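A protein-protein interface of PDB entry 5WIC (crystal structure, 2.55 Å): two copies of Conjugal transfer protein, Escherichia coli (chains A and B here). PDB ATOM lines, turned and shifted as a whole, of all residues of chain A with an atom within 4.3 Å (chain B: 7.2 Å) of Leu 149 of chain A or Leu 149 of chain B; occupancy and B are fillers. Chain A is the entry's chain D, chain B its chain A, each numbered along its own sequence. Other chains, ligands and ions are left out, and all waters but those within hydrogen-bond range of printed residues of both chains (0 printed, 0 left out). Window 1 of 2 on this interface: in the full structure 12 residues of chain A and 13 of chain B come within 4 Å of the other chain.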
ATOM      1  N   TYR A  25       0.067 -23.612  24.677  1.00  0.00           N
ATOM      2  CA  TYR A  25       0.842 -24.038  25.837  1.00  0.00           C
ATOM      3  C   TYR A  25       0.621 -23.126  27.039  1.00  0.00           C
ATOM      4  O   TYR A  25       1.217 -23.331  28.092  1.00  0.00           O
ATOM      5  CB  TYR A  25       2.332 -24.081  25.494  1.00  0.00           C
ATOM      6  CG  TYR A  25       2.838 -25.453  25.116  1.00  0.00           C
ATOM      7  CD1 TYR A  25       2.916 -26.466  26.060  1.00  0.00           C
ATOM      8  CD2 TYR A  25       3.248 -25.732  23.821  1.00  0.00           C
ATOM      9  CE1 TYR A  25       3.380 -27.721  25.724  1.00  0.00           C
ATOM     10  CE2 TYR A  25       3.714 -26.986  23.475  1.00  0.00           C
ATOM     11  CZ  TYR A  25       3.778 -27.976  24.430  1.00  0.00           C
ATOM     12  OH  TYR A  25       4.242 -29.226  24.092  1.00  0.00           O
ATOM     13  N   ILE A  29       3.856 -18.944  28.863  1.00  0.00           N
ATOM     14  CA  ILE A  29       4.818 -19.754  28.134  1.00  0.00           C
ATOM     15  C   ILE A  29       4.950 -19.239  26.703  1.00  0.00           C
ATOM     16  O   ILE A  29       6.049 -19.196  26.153  1.00  0.00           O
ATOM     17  CB  ILE A  29       4.414 -21.239  28.137  1.00  0.00           C
ATOM     18  CG1 ILE A  29       4.344 -21.741  29.585  1.00  0.00           C
ATOM     19  CG2 ILE A  29       5.401 -22.063  27.308  1.00  0.00           C
ATOM     20  CD1 ILE A  29       4.085 -23.228  29.746  1.00  0.00           C
ATOM     21  N   TRP A  33       8.762 -17.429  24.769  1.00  0.00           N
ATOM     22  CA  TRP A  33       9.396 -17.773  23.531  1.00  0.00           C
ATOM     23  C   TRP A  33       9.344 -16.680  22.540  1.00  0.00           C
ATOM     24  O   TRP A  33      10.313 -16.420  21.855  1.00  0.00           O
ATOM     25  CB  TRP A  33       8.770 -19.011  22.960  1.00  0.00           C
ATOM     26  CG  TRP A  33       8.977 -20.190  23.836  1.00  0.00           C
ATOM     27  CD1 TRP A  33       8.032 -20.899  24.528  1.00  0.00           C
ATOM     28  CD2 TRP A  33      10.222 -20.829  24.154  1.00  0.00           C
ATOM     29  NE1 TRP A  33       8.597 -21.906  25.228  1.00  0.00           N
ATOM     30  CE2 TRP A  33       9.901 -21.919  25.048  1.00  0.00           C
ATOM     31  CE3 TRP A  33      11.518 -20.624  23.801  1.00  0.00           C
ATOM     32  CZ2 TRP A  33      10.852 -22.741  25.556  1.00  0.00           C
ATOM     33  CZ3 TRP A  33      12.471 -21.464  24.318  1.00  0.00           C
ATOM     34  CH2 TRP A  33      12.143 -22.498  25.178  1.00  0.00           C
ATOM     35  N   TYR A 134       3.370 -24.531  17.594  1.00  0.00           N
ATOM     36  CA  TYR A 134       4.200 -25.522  18.274  1.00  0.00           C
ATOM     37  C   TYR A 134       4.179 -26.870  17.559  1.00  0.00           C
ATOM     38  O   TYR A 134       3.115 -27.431  17.297  1.00  0.00           O
ATOM     39  CB  TYR A 134       3.737 -25.703  19.721  1.00  0.00           C
ATOM     40  CG  TYR A 134       3.953 -24.493  20.601  1.00  0.00           C
ATOM     41  CD1 TYR A 134       3.004 -23.482  20.672  1.00  0.00           C
ATOM     42  CD2 TYR A 134       5.102 -24.367  21.370  1.00  0.00           C
ATOM     43  CE1 TYR A 134       3.196 -22.377  21.480  1.00  0.00           C
ATOM     44  CE2 TYR A 134       5.303 -23.266  22.179  1.00  0.00           C
ATOM     45  CZ  TYR A 134       4.347 -22.274  22.231  1.00  0.00           C
ATOM     46  OH  TYR A 134       4.541 -21.176  23.038  1.00  0.00           O
ATOM     47  N   LYS A 135       5.367 -27.383  17.253  1.00  0.00           N
ATOM     48  CA  LYS A 135       5.522 -28.710  16.665  1.00  0.00           C
ATOM     49  C   LYS A 135       6.854 -29.319  17.089  1.00  0.00           C
ATOM     50  O   LYS A 135       7.863 -29.159  16.405  1.00  0.00           O
ATOM     51  CB  LYS A 135       5.441 -28.648  15.136  1.00  0.00           C
ATOM     52  CG  LYS A 135       4.053 -28.362  14.587  1.00  0.00           C
ATOM     53  CD  LYS A 135       4.040 -28.399  13.070  1.00  0.00           C
ATOM     54  CE  LYS A 135       2.648 -28.143  12.521  1.00  0.00           C
ATOM     55  NZ  LYS A 135       2.628 -28.144  11.033  1.00  0.00           N
ATOM     56  N   SER A 136       6.855 -30.012  18.223  1.00  0.00           N
ATOM     57  CA  SER A 136       8.069 -30.650  18.721  1.00  0.00           C
ATOM     58  C   SER A 136       8.406 -31.876  17.878  1.00  0.00           C
ATOM     59  O   SER A 136       7.844 -32.954  18.082  1.00  0.00           O
ATOM     60  CB  SER A 136       7.906 -31.042  20.192  1.00  0.00           C
ATOM     61  OG  SER A 136       9.094 -31.627  20.695  1.00  0.00           O
ATOM     62  N   ASN A 147      15.044 -24.839  21.891  1.00  0.00           N
ATOM     63  CA  ASN A 147      13.605 -24.938  21.688  1.00  0.00           C
ATOM     64  C   ASN A 147      13.040 -26.310  22.057  1.00  0.00           C
ATOM     65  O   ASN A 147      12.786 -27.119  21.211  1.00  0.00           O
ATOM     66  CB  ASN A 147      13.210 -24.572  20.254  1.00  0.00           C
ATOM     67  CG  ASN A 147      11.752 -24.227  20.121  1.00  0.00           C
ATOM     68  OD1 ASN A 147      11.022 -24.229  21.084  1.00  0.00           O
ATOM     69  ND2 ASN A 147      11.324 -23.929  18.924  1.00  0.00           N
ATOM     70  N   PRO A 148      12.830 -26.563  23.324  1.00  0.00           N
ATOM     71  CA  PRO A 148      12.303 -27.854  23.775  1.00  0.00           C
ATOM     72  C   PRO A 148      10.849 -28.084  23.376  1.00  0.00           C
ATOM     73  O   PRO A 148      10.460 -29.229  23.162  1.00  0.00           O
ATOM     74  CB  PRO A 148      12.436 -27.777  25.302  1.00  0.00           C
ATOM     75  CG  PRO A 148      13.385 -26.662  25.567  1.00  0.00           C
ATOM     76  CD  PRO A 148      13.167 -25.692  24.461  1.00  0.00           C
ATOM     77  N   LEU A 149      10.060 -27.018  23.283  1.00  0.00           N
ATOM     78  CA  LEU A 149       8.639 -27.151  22.980  1.00  0.00           C
ATOM     79  C   LEU A 149       8.367 -27.131  21.481  1.00  0.00           C
ATOM     80  O   LEU A 149       7.234 -27.343  21.047  1.00  0.00           O
ATOM     81  CB  LEU A 149       7.838 -26.038  23.660  1.00  0.00           C
ATOM     82  CG  LEU A 149       7.916 -25.947  25.186  1.00  0.00           C
ATOM     83  CD1 LEU A 149       6.858 -24.985  25.696  1.00  0.00           C
ATOM     84  CD2 LEU A 149       7.759 -27.305  25.849  1.00  0.00           C
ATOM     85  N   GLY A 150       9.403 -26.877  20.690  1.00  0.00           N
ATOM     86  CA  GLY A 150       9.251 -26.817  19.249  1.00  0.00           C
ATOM     87  C   GLY A 150       8.480 -25.588  18.813  1.00  0.00           C
ATOM     88  O   GLY A 150       7.698 -25.635  17.865  1.00  0.00           O
ATOM     89  N   PHE A 151       8.694 -24.484  19.521  1.00  0.00           N
ATOM     90  CA  PHE A 151       8.117 -23.200  19.140  1.00  0.00           C
ATOM     91  C   PHE A 151       8.705 -22.730  17.813  1.00  0.00           C
ATOM     92  O   PHE A 151       9.905 -22.865  17.581  1.00  0.00           O
ATOM     93  CB  PHE A 151       8.371 -22.165  20.236  1.00  0.00           C
ATOM     94  CG  PHE A 151       8.129 -20.748  19.804  1.00  0.00           C
ATOM     95  CD1 PHE A 151       6.872 -20.183  19.902  1.00  0.00           C
ATOM     96  CD2 PHE A 151       9.165 -19.977  19.308  1.00  0.00           C
ATOM     97  CE1 PHE A 151       6.652 -18.880  19.510  1.00  0.00           C
ATOM     98  CE2 PHE A 151       8.951 -18.676  18.912  1.00  0.00           C
ATOM     99  CZ  PHE A 151       7.693 -18.126  19.014  1.00  0.00           C
ATOM    100  N   THR B  19       9.102 -34.260  30.640  1.00  0.00           N
ATOM    101  CA  THR B  19       9.273 -35.196  29.534  1.00  0.00           C
ATOM    102  C   THR B  19      10.699 -35.750  29.470  1.00  0.00           C
ATOM    103  O   THR B  19      10.961 -36.705  28.739  1.00  0.00           O
ATOM    104  CB  THR B  19       8.936 -34.535  28.183  1.00  0.00           C
ATOM    105  OG1 THR B  19       9.025 -35.507  27.131  1.00  0.00           O
ATOM    106  CG2 THR B  19       9.884 -33.379  27.893  1.00  0.00           C
ATOM    107  N   ARG B  20      11.615 -35.147  30.225  1.00  0.00           N
ATOM    108  CA  ARG B  20      12.993 -35.632  30.289  1.00  0.00           C
ATOM    109  C   ARG B  20      13.662 -35.257  31.610  1.00  0.00           C
ATOM    110  O   ARG B  20      13.592 -34.112  32.050  1.00  0.00           O
ATOM    111  CB  ARG B  20      13.808 -35.081  29.117  1.00  0.00           C
ATOM    112  CG  ARG B  20      15.233 -35.609  29.056  1.00  0.00           C
ATOM    113  CD  ARG B  20      15.923 -35.212  27.763  1.00  0.00           C
ATOM    114  NE  ARG B  20      17.250 -35.817  27.656  1.00  0.00           N
ATOM    115  CZ  ARG B  20      18.377 -35.258  28.090  1.00  0.00           C
ATOM    116  NH1 ARG B  20      18.362 -34.063  28.664  1.00  0.00           N
ATOM    117  NH2 ARG B  20      19.528 -35.898  27.947  1.00  0.00           N
ATOM    118  N   ASP B  21      14.313 -36.231  32.238  1.00  0.00           N
ATOM    119  CA  ASP B  21      15.036 -35.990  33.480  1.00  0.00           C
ATOM    120  C   ASP B  21      16.319 -35.202  33.234  1.00  0.00           C
ATOM    121  O   ASP B  21      17.232 -35.688  32.573  1.00  0.00           O
ATOM    122  CB  ASP B  21      15.380 -37.312  34.175  1.00  0.00           C
ATOM    123  CG  ASP B  21      14.152 -38.122  34.546  1.00  0.00           C
ATOM    124  OD1 ASP B  21      13.049 -37.544  34.625  1.00  0.00           O
ATOM    125  OD2 ASP B  21      14.293 -39.345  34.766  1.00  0.00           O
ATOM    126  N   GLN B  22      16.381 -33.985  33.769  1.00  0.00           N
ATOM    127  CA  GLN B  22      17.607 -33.188  33.750  1.00  0.00           C
ATOM    128  C   GLN B  22      17.500 -32.036  34.745  1.00  0.00           C
ATOM    129  O   GLN B  22      16.423 -31.487  34.958  1.00  0.00           O
ATOM    130  CB  GLN B  22      17.893 -32.648  32.347  1.00  0.00           C
ATOM    131  CG  GLN B  22      16.873 -31.648  31.837  1.00  0.00           C
ATOM    132  CD  GLN B  22      16.950 -31.455  30.334  1.00  0.00           C
ATOM    133  OE1 GLN B  22      16.673 -32.376  29.566  1.00  0.00           O
ATOM    134  NE2 GLN B  22      17.326 -30.253  29.906  1.00  0.00           N
ATOM    135  N   TYR B  25      17.882 -26.541  32.013  1.00  0.00           N
ATOM    136  CA  TYR B  25      17.583 -26.313  30.603  1.00  0.00           C
ATOM    137  C   TYR B  25      18.282 -25.046  30.111  1.00  0.00           C
ATOM    138  O   TYR B  25      17.939 -24.501  29.065  1.00  0.00           O
ATOM    139  CB  TYR B  25      16.072 -26.199  30.384  1.00  0.00           C
ATOM    140  CG  TYR B  25      15.417 -27.484  29.938  1.00  0.00           C
ATOM    141  CD1 TYR B  25      15.329 -27.808  28.592  1.00  0.00           C
ATOM    142  CD2 TYR B  25      14.883 -28.373  30.863  1.00  0.00           C
ATOM    143  CE1 TYR B  25      14.731 -28.983  28.179  1.00  0.00           C
ATOM    144  CE2 TYR B  25      14.284 -29.548  30.460  1.00  0.00           C
ATOM    145  CZ  TYR B  25      14.210 -29.848  29.117  1.00  0.00           C
ATOM    146  OH  TYR B  25      13.611 -31.017  28.716  1.00  0.00           O
ATOM    147  N   ILE B  29      15.846 -20.468  30.306  1.00  0.00           N
ATOM    148  CA  ILE B  29      14.704 -21.357  30.475  1.00  0.00           C
ATOM    149  C   ILE B  29      14.490 -21.635  31.958  1.00  0.00           C
ATOM    150  O   ILE B  29      13.359 -21.607  32.441  1.00  0.00           O
ATOM    151  CB  ILE B  29      14.888 -22.680  29.702  1.00  0.00           C
ATOM    152  CG1 ILE B  29      15.094 -22.379  28.214  1.00  0.00           C
ATOM    153  CG2 ILE B  29      13.677 -23.593  29.912  1.00  0.00           C
ATOM    154  CD1 ILE B  29      15.249 -23.600  27.326  1.00  0.00           C
ATOM    155  N   TRP B  33      10.915 -20.500  34.527  1.00  0.00           N
ATOM    156  CA  TRP B  33      10.157 -21.320  35.415  1.00  0.00           C
ATOM    157  C   TRP B  33      10.297 -20.923  36.833  1.00  0.00           C
ATOM    158  O   TRP B  33       9.334 -20.870  37.565  1.00  0.00           O
ATOM    159  CB  TRP B  33      10.510 -22.789  35.226  1.00  0.00           C
ATOM    160  CG  TRP B  33      10.189 -23.303  33.858  1.00  0.00           C
ATOM    161  CD1 TRP B  33      11.064 -23.712  32.890  1.00  0.00           C
ATOM    162  CD2 TRP B  33       8.886 -23.461  33.256  1.00  0.00           C
ATOM    163  NE1 TRP B  33      10.415 -24.081  31.778  1.00  0.00           N
ATOM    164  CE2 TRP B  33       9.112 -23.954  31.931  1.00  0.00           C
ATOM    165  CE3 TRP B  33       7.613 -23.236  33.662  1.00  0.00           C
ATOM    166  CZ2 TRP B  33       8.089 -24.216  31.077  1.00  0.00           C
ATOM    167  CZ3 TRP B  33       6.592 -23.496  32.793  1.00  0.00           C
ATOM    168  CH2 TRP B  33       6.825 -23.979  31.536  1.00  0.00           C
ATOM    169  N   GLU B 133      14.645 -28.945  39.525  1.00  0.00           N
ATOM    170  CA  GLU B 133      14.990 -30.055  38.643  1.00  0.00           C
ATOM    171  C   GLU B 133      13.926 -30.202  37.557  1.00  0.00           C
ATOM    172  O   GLU B 133      12.876 -29.564  37.625  1.00  0.00           O
ATOM    173  CB  GLU B 133      15.109 -31.354  39.440  1.00  0.00           C
ATOM    174  CG  GLU B 133      13.782 -31.882  39.963  1.00  0.00           C
ATOM    175  CD  GLU B 133      13.946 -33.123  40.819  1.00  0.00           C
ATOM    176  OE1 GLU B 133      15.097 -33.573  41.003  1.00  0.00           O
ATOM    177  OE2 GLU B 133      12.924 -33.648  41.308  1.00  0.00           O
ATOM    178  N   TYR B 134      14.186 -31.050  36.570  1.00  0.00           N
ATOM    179  CA  TYR B 134      13.149 -31.429  35.623  1.00  0.00           C
ATOM    180  C   TYR B 134      13.017 -32.937  35.651  1.00  0.00           C
ATOM    181  O   TYR B 134      14.015 -33.655  35.736  1.00  0.00           O
ATOM    182  CB  TYR B 134      13.468 -30.945  34.210  1.00  0.00           C
ATOM    183  CG  TYR B 134      13.609 -29.446  34.068  1.00  0.00           C
ATOM    184  CD1 TYR B 134      14.767 -28.795  34.465  1.00  0.00           C
ATOM    185  CD2 TYR B 134      12.591 -28.686  33.511  1.00  0.00           C
ATOM    186  CE1 TYR B 134      14.904 -27.428  34.320  1.00  0.00           C
ATOM    187  CE2 TYR B 134      12.718 -27.317  33.363  1.00  0.00           C
ATOM    188  CZ  TYR B 134      13.877 -26.695  33.769  1.00  0.00           C
ATOM    189  OH  TYR B 134      14.011 -25.334  33.622  1.00  0.00           O
ATOM    190  N   LYS B 135      11.779 -33.412  35.596  1.00  0.00           N
ATOM    191  CA  LYS B 135      11.510 -34.839  35.636  1.00  0.00           C
ATOM    192  C   LYS B 135      10.534 -35.239  34.546  1.00  0.00           C
ATOM    193  O   LYS B 135       9.562 -34.537  34.269  1.00  0.00           O
ATOM    194  CB  LYS B 135      10.963 -35.243  37.005  1.00  0.00           C
ATOM    195  CG  LYS B 135      11.988 -35.195  38.122  1.00  0.00           C
ATOM    196  CD  LYS B 135      13.045 -36.280  37.973  1.00  0.00           C
ATOM    197  CE  LYS B 135      14.053 -36.228  39.113  1.00  0.00           C
ATOM    198  NZ  LYS B 135      15.254 -37.074  38.863  1.00  0.00           N
ATOM    199  N   SER B 136      10.820 -36.371  33.917  1.00  0.00           N
ATOM    200  CA  SER B 136       9.895 -36.987  32.984  1.00  0.00           C
ATOM    201  C   SER B 136       8.856 -37.770  33.774  1.00  0.00           C
ATOM    202  O   SER B 136       9.182 -38.769  34.415  1.00  0.00           O
ATOM    203  CB  SER B 136      10.638 -37.900  32.011  1.00  0.00           C
ATOM    204  OG  SER B 136      11.340 -38.917  32.706  1.00  0.00           O
ATOM    205  N   LEU B 137       7.614 -37.301  33.742  1.00  0.00           N
ATOM    206  CA  LEU B 137       6.532 -37.956  34.465  1.00  0.00           C
ATOM    207  C   LEU B 137       5.282 -38.059  33.605  1.00  0.00           C
ATOM    208  O   LEU B 137       5.121 -37.322  32.631  1.00  0.00           O
ATOM    209  CB  LEU B 137       6.211 -37.196  35.755  1.00  0.00           C
ATOM    210  CG  LEU B 137       7.303 -37.166  36.827  1.00  0.00           C
ATOM    211  CD1 LEU B 137       6.878 -36.274  37.982  1.00  0.00           C
ATOM    212  CD2 LEU B 137       7.620 -38.564  37.331  1.00  0.00           C
ATOM    213  N   MET B 139       1.728 -37.276  32.509  1.00  0.00           N
ATOM    214  CA  MET B 139       1.132 -35.949  32.552  1.00  0.00           C
ATOM    215  C   MET B 139      -0.037 -35.865  31.575  1.00  0.00           C
ATOM    216  O   MET B 139       0.114 -36.178  30.397  1.00  0.00           O
ATOM    217  CB  MET B 139       2.199 -34.902  32.221  1.00  0.00           C
ATOM    218  CG  MET B 139       2.061 -33.586  32.966  1.00  0.00           C
ATOM    219  SD  MET B 139       3.551 -32.572  32.867  1.00  0.00           S
ATOM    220  CE  MET B 139       4.699 -33.511  33.870  1.00  0.00           C
ATOM    221  N   GLN B 143      -2.333 -30.691  32.142  1.00  0.00           N
ATOM    222  CA  GLN B 143      -1.148 -30.649  32.996  1.00  0.00           C
ATOM    223  C   GLN B 143       0.089 -30.247  32.197  1.00  0.00           C
ATOM    224  O   GLN B 143       0.859 -29.389  32.624  1.00  0.00           O
ATOM    225  CB  GLN B 143      -0.906 -32.001  33.665  1.00  0.00           C
ATOM    226  CG  GLN B 143      -1.768 -32.268  34.880  1.00  0.00           C
ATOM    227  CD  GLN B 143      -1.519 -33.639  35.469  1.00  0.00           C
ATOM    228  OE1 GLN B 143      -0.937 -34.507  34.820  1.00  0.00           O
ATOM    229  NE2 GLN B 143      -1.949 -33.840  36.709  1.00  0.00           N
ATOM    230  N   ARG B 144       0.283 -30.880  31.044  1.00  0.00           N
ATOM    231  CA  ARG B 144       1.381 -30.521  30.152  1.00  0.00           C
ATOM    232  C   ARG B 144       1.215 -29.090  29.660  1.00  0.00           C
ATOM    233  O   ARG B 144       2.185 -28.426  29.307  1.00  0.00           O
ATOM    234  CB  ARG B 144       1.447 -31.471  28.955  1.00  0.00           C
ATOM    235  CG  ARG B 144       1.742 -32.914  29.312  1.00  0.00           C
ATOM    236  CD  ARG B 144       1.912 -33.773  28.065  1.00  0.00           C
ATOM    237  NE  ARG B 144       1.039 -33.355  26.968  1.00  0.00           N
ATOM    238  CZ  ARG B 144      -0.207 -33.785  26.779  1.00  0.00           C
ATOM    239  NH1 ARG B 144      -0.759 -34.654  27.616  1.00  0.00           N
ATOM    240  NH2 ARG B 144      -0.909 -33.339  25.745  1.00  0.00           N
ATOM    241  N   VAL B 146       0.533 -26.673  31.373  1.00  0.00           N
ATOM    242  CA  VAL B 146       0.961 -25.769  32.438  1.00  0.00           C
ATOM    243  C   VAL B 146       2.431 -25.986  32.785  1.00  0.00           C
ATOM    244  O   VAL B 146       3.146 -25.033  33.089  1.00  0.00           O
ATOM    245  CB  VAL B 146       0.097 -25.952  33.705  1.00  0.00           C
ATOM    246  CG1 VAL B 146       0.621 -25.102  34.854  1.00  0.00           C
ATOM    247  CG2 VAL B 146      -1.347 -25.595  33.407  1.00  0.00           C
ATOM    248  N   ASN B 147       2.874 -27.238  32.733  1.00  0.00           N
ATOM    249  CA  ASN B 147       4.241 -27.590  33.099  1.00  0.00           C
ATOM    250  C   ASN B 147       4.843 -28.589  32.108  1.00  0.00           C
ATOM    251  O   ASN B 147       5.217 -29.697  32.489  1.00  0.00           O
ATOM    252  CB  ASN B 147       4.266 -28.161  34.518  1.00  0.00           C
ATOM    253  CG  ASN B 147       5.665 -28.256  35.088  1.00  0.00           C
ATOM    254  OD1 ASN B 147       6.556 -27.504  34.705  1.00  0.00           O
ATOM    255  ND2 ASN B 147       5.863 -29.187  36.013  1.00  0.00           N
ATOM    256  N   PRO B 148       4.956 -28.183  30.832  1.00  0.00           N
ATOM    257  CA  PRO B 148       5.331 -29.084  29.732  1.00  0.00           C
ATOM    258  C   PRO B 148       6.630 -29.843  29.973  1.00  0.00           C
ATOM    259  O   PRO B 148       6.716 -31.032  29.664  1.00  0.00           O
ATOM    260  CB  PRO B 148       5.495 -28.139  28.536  1.00  0.00           C
ATOM    261  CG  PRO B 148       4.818 -26.876  28.912  1.00  0.00           C
ATOM    262  CD  PRO B 148       4.885 -26.779  30.395  1.00  0.00           C
ATOM    263  N   LEU B 149       7.627 -29.157  30.520  1.00  0.00           N
ATOM    264  CA  LEU B 149       8.955 -29.736  30.681  1.00  0.00           C
ATOM    265  C   LEU B 149       9.108 -30.459  32.013  1.00  0.00           C
ATOM    266  O   LEU B 149      10.184 -30.964  32.330  1.00  0.00           O
ATOM    267  CB  LEU B 149      10.017 -28.646  30.557  1.00  0.00           C
ATOM    268  CG  LEU B 149       9.948 -27.802  29.282  1.00  0.00           C
ATOM    269  CD1 LEU B 149      11.061 -26.776  29.282  1.00  0.00           C
ATOM    270  CD2 LEU B 149      10.031 -28.673  28.040  1.00  0.00           C
ATOM    271  N   GLY B 150       8.032 -30.509  32.790  1.00  0.00           N
ATOM    272  CA  GLY B 150       8.050 -31.211  34.059  1.00  0.00           C
ATOM    273  C   GLY B 150       8.938 -30.539  35.091  1.00  0.00           C
ATOM    274  O   GLY B 150       9.533 -31.204  35.940  1.00  0.00           O
ATOM    275  N   PHE B 151       9.029 -29.214  35.017  1.00  0.00           N
ATOM    276  CA  PHE B 151       9.794 -28.448  35.993  1.00  0.00           C
ATOM    277  C   PHE B 151       9.196 -28.642  37.375  1.00  0.00           C
ATOM    278  O   PHE B 151       7.976 -28.679  37.525  1.00  0.00           O
ATOM    279  CB  PHE B 151       9.809 -26.963  35.622  1.00  0.00           C
ATOM    280  CG  PHE B 151      10.384 -26.072  36.689  1.00  0.00           C
ATOM    281  CD1 PHE B 151      11.749 -25.844  36.764  1.00  0.00           C
ATOM    282  CD2 PHE B 151       9.556 -25.447  37.609  1.00  0.00           C
ATOM    283  CE1 PHE B 151      12.279 -25.017  37.744  1.00  0.00           C
ATOM    284  CE2 PHE B 151      10.077 -24.625  38.585  1.00  0.00           C
ATOM    285  CZ  PHE B 151      11.441 -24.409  38.653  1.00  0.00           C
ATOM    286  N   ARG B 152      10.048 -28.785  38.382  1.00  0.00           N
ATOM    287  CA  ARG B 152       9.566 -28.831  39.752  1.00  0.00           C
ATOM    288  C   ARG B 152      10.611 -28.351  40.755  1.00  0.00           C
ATOM    289  O   ARG B 152      11.807 -28.600  40.606  1.00  0.00           O
ATOM    290  CB  ARG B 152       9.103 -30.245  40.106  1.00  0.00           C
ATOM    291  CG  ARG B 152      10.212 -31.230  40.404  1.00  0.00           C
ATOM    292  CD  ARG B 152       9.630 -32.603  40.694  1.00  0.00           C
ATOM    293  NE  ARG B 152      10.640 -33.546  41.165  1.00  0.00           N
ATOM    294  CZ  ARG B 152      10.381 -34.801  41.518  1.00  0.00           C
ATOM    295  NH1 ARG B 152       9.141 -35.272  41.456  1.00  0.00           N
ATOM    296  NH2 ARG B 152      11.364 -35.587  41.938  1.00  0.00           N
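The guanidinium group (NH1) of Arg 144 of chain B lies within hydrogen-bond range of the backbone carbonyl oxygen (O) of Met 139 of chain B (3.3 Å).
OE1 of Gln 22 of chain B lies within hydrogen-bond range of OH of Tyr 25 of chain B, 3.5 Å away.
Tyr 25 of chain A touches Pro 148 of chain B, and with the chains exchanged Pro 148 of chain A touches Tyr 25 of chain B.
Ile 29 of chain A touches Trp 33 of chain B, and with the chains exchanged Trp 33 of chain A touches Ile 29 of chain B.
Ile 29 of chain A touches Pro 148 of chain B, and with the chains exchanged Pro 148 of chain A touches Ile 29 of chain B.
Pro 148 of chain A touches Leu 149 of chain B, and with the chains exchanged Leu 149 of chain A touches Pro 148 of chain B.
Of chain B, only Pro 148 (3.6 Å) and Leu 149 (3.4 Å) come within 4 Å of Leu 149 of chain A.
Of chain A, only Pro 148 (3.8 Å) and Leu 149 (3.4 Å) come within 4 Å of Leu 149 of chain B.
Of the printed residues of chain A, Ile 29 of chain B touches Trp 33 (3.9 Å) and Pro 148 (3.99 Å).
Of the printed residues of chain B, Pro 148 of chain A touches Tyr 25, Ile 29 and Leu 149.
The nearest printed residue of chain A that does not touch Leu 149 of chain B is Trp 33 of chain A (5.5 Å).
The nearest printed residue of chain A that does not touch Trp 33 of chain B is Leu 149 of chain A (5.6 Å).
Hydrophobic or aromatic side chains of chain B within 4 Å of the printed part of chain A: Tyr 25, Ile 29, Trp 33, Pro 148 and Leu 149.
Of the 11 printed residues of chain A, 5 touch a printed residue of chain B.
Hydrophobic or aromatic side chains of chain A within 4 Å of the printed part of chain B: Tyr 25, Ile 29, Trp 33, Pro 148 and Leu 149.
Among the printed residues, 11 pairs touch across the chains.
Among the printed residues, no Asp or Glu carboxylate lies within 4 Å of a Lys or Arg side-chain nitrogen of the other chain.
Among the printed residues, pairs that only touch across the chains: Ile 29 of chain A with Trp 33 of chain B (3.4 Å), Leu 149 of chain A with Leu 149 of chain B (3.4 Å), Tyr 25 of chain A with Pro 148 of chain B (3.5 Å), Leu 149 of chain A with Pro 148 of chain B (3.6 Å), Ile 29 of chain A with Pro 148 of chain B (3.7 Å), Pro 148 of chain A with Tyr 25 of chain B (3.7 Å), Pro 148 of chain A with Leu 149 of chain B (3.8 Å), Tyr 25 of chain A with Arg 144 of chain B (3.8 Å), Ile 29 of chain A with Val 146 of chain B (3.9 Å), Trp 33 of chain A with Ile 29 of chain B (3.9 Å) and Pro 148 of chain A with Ile 29 of chain B (3.99 Å).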
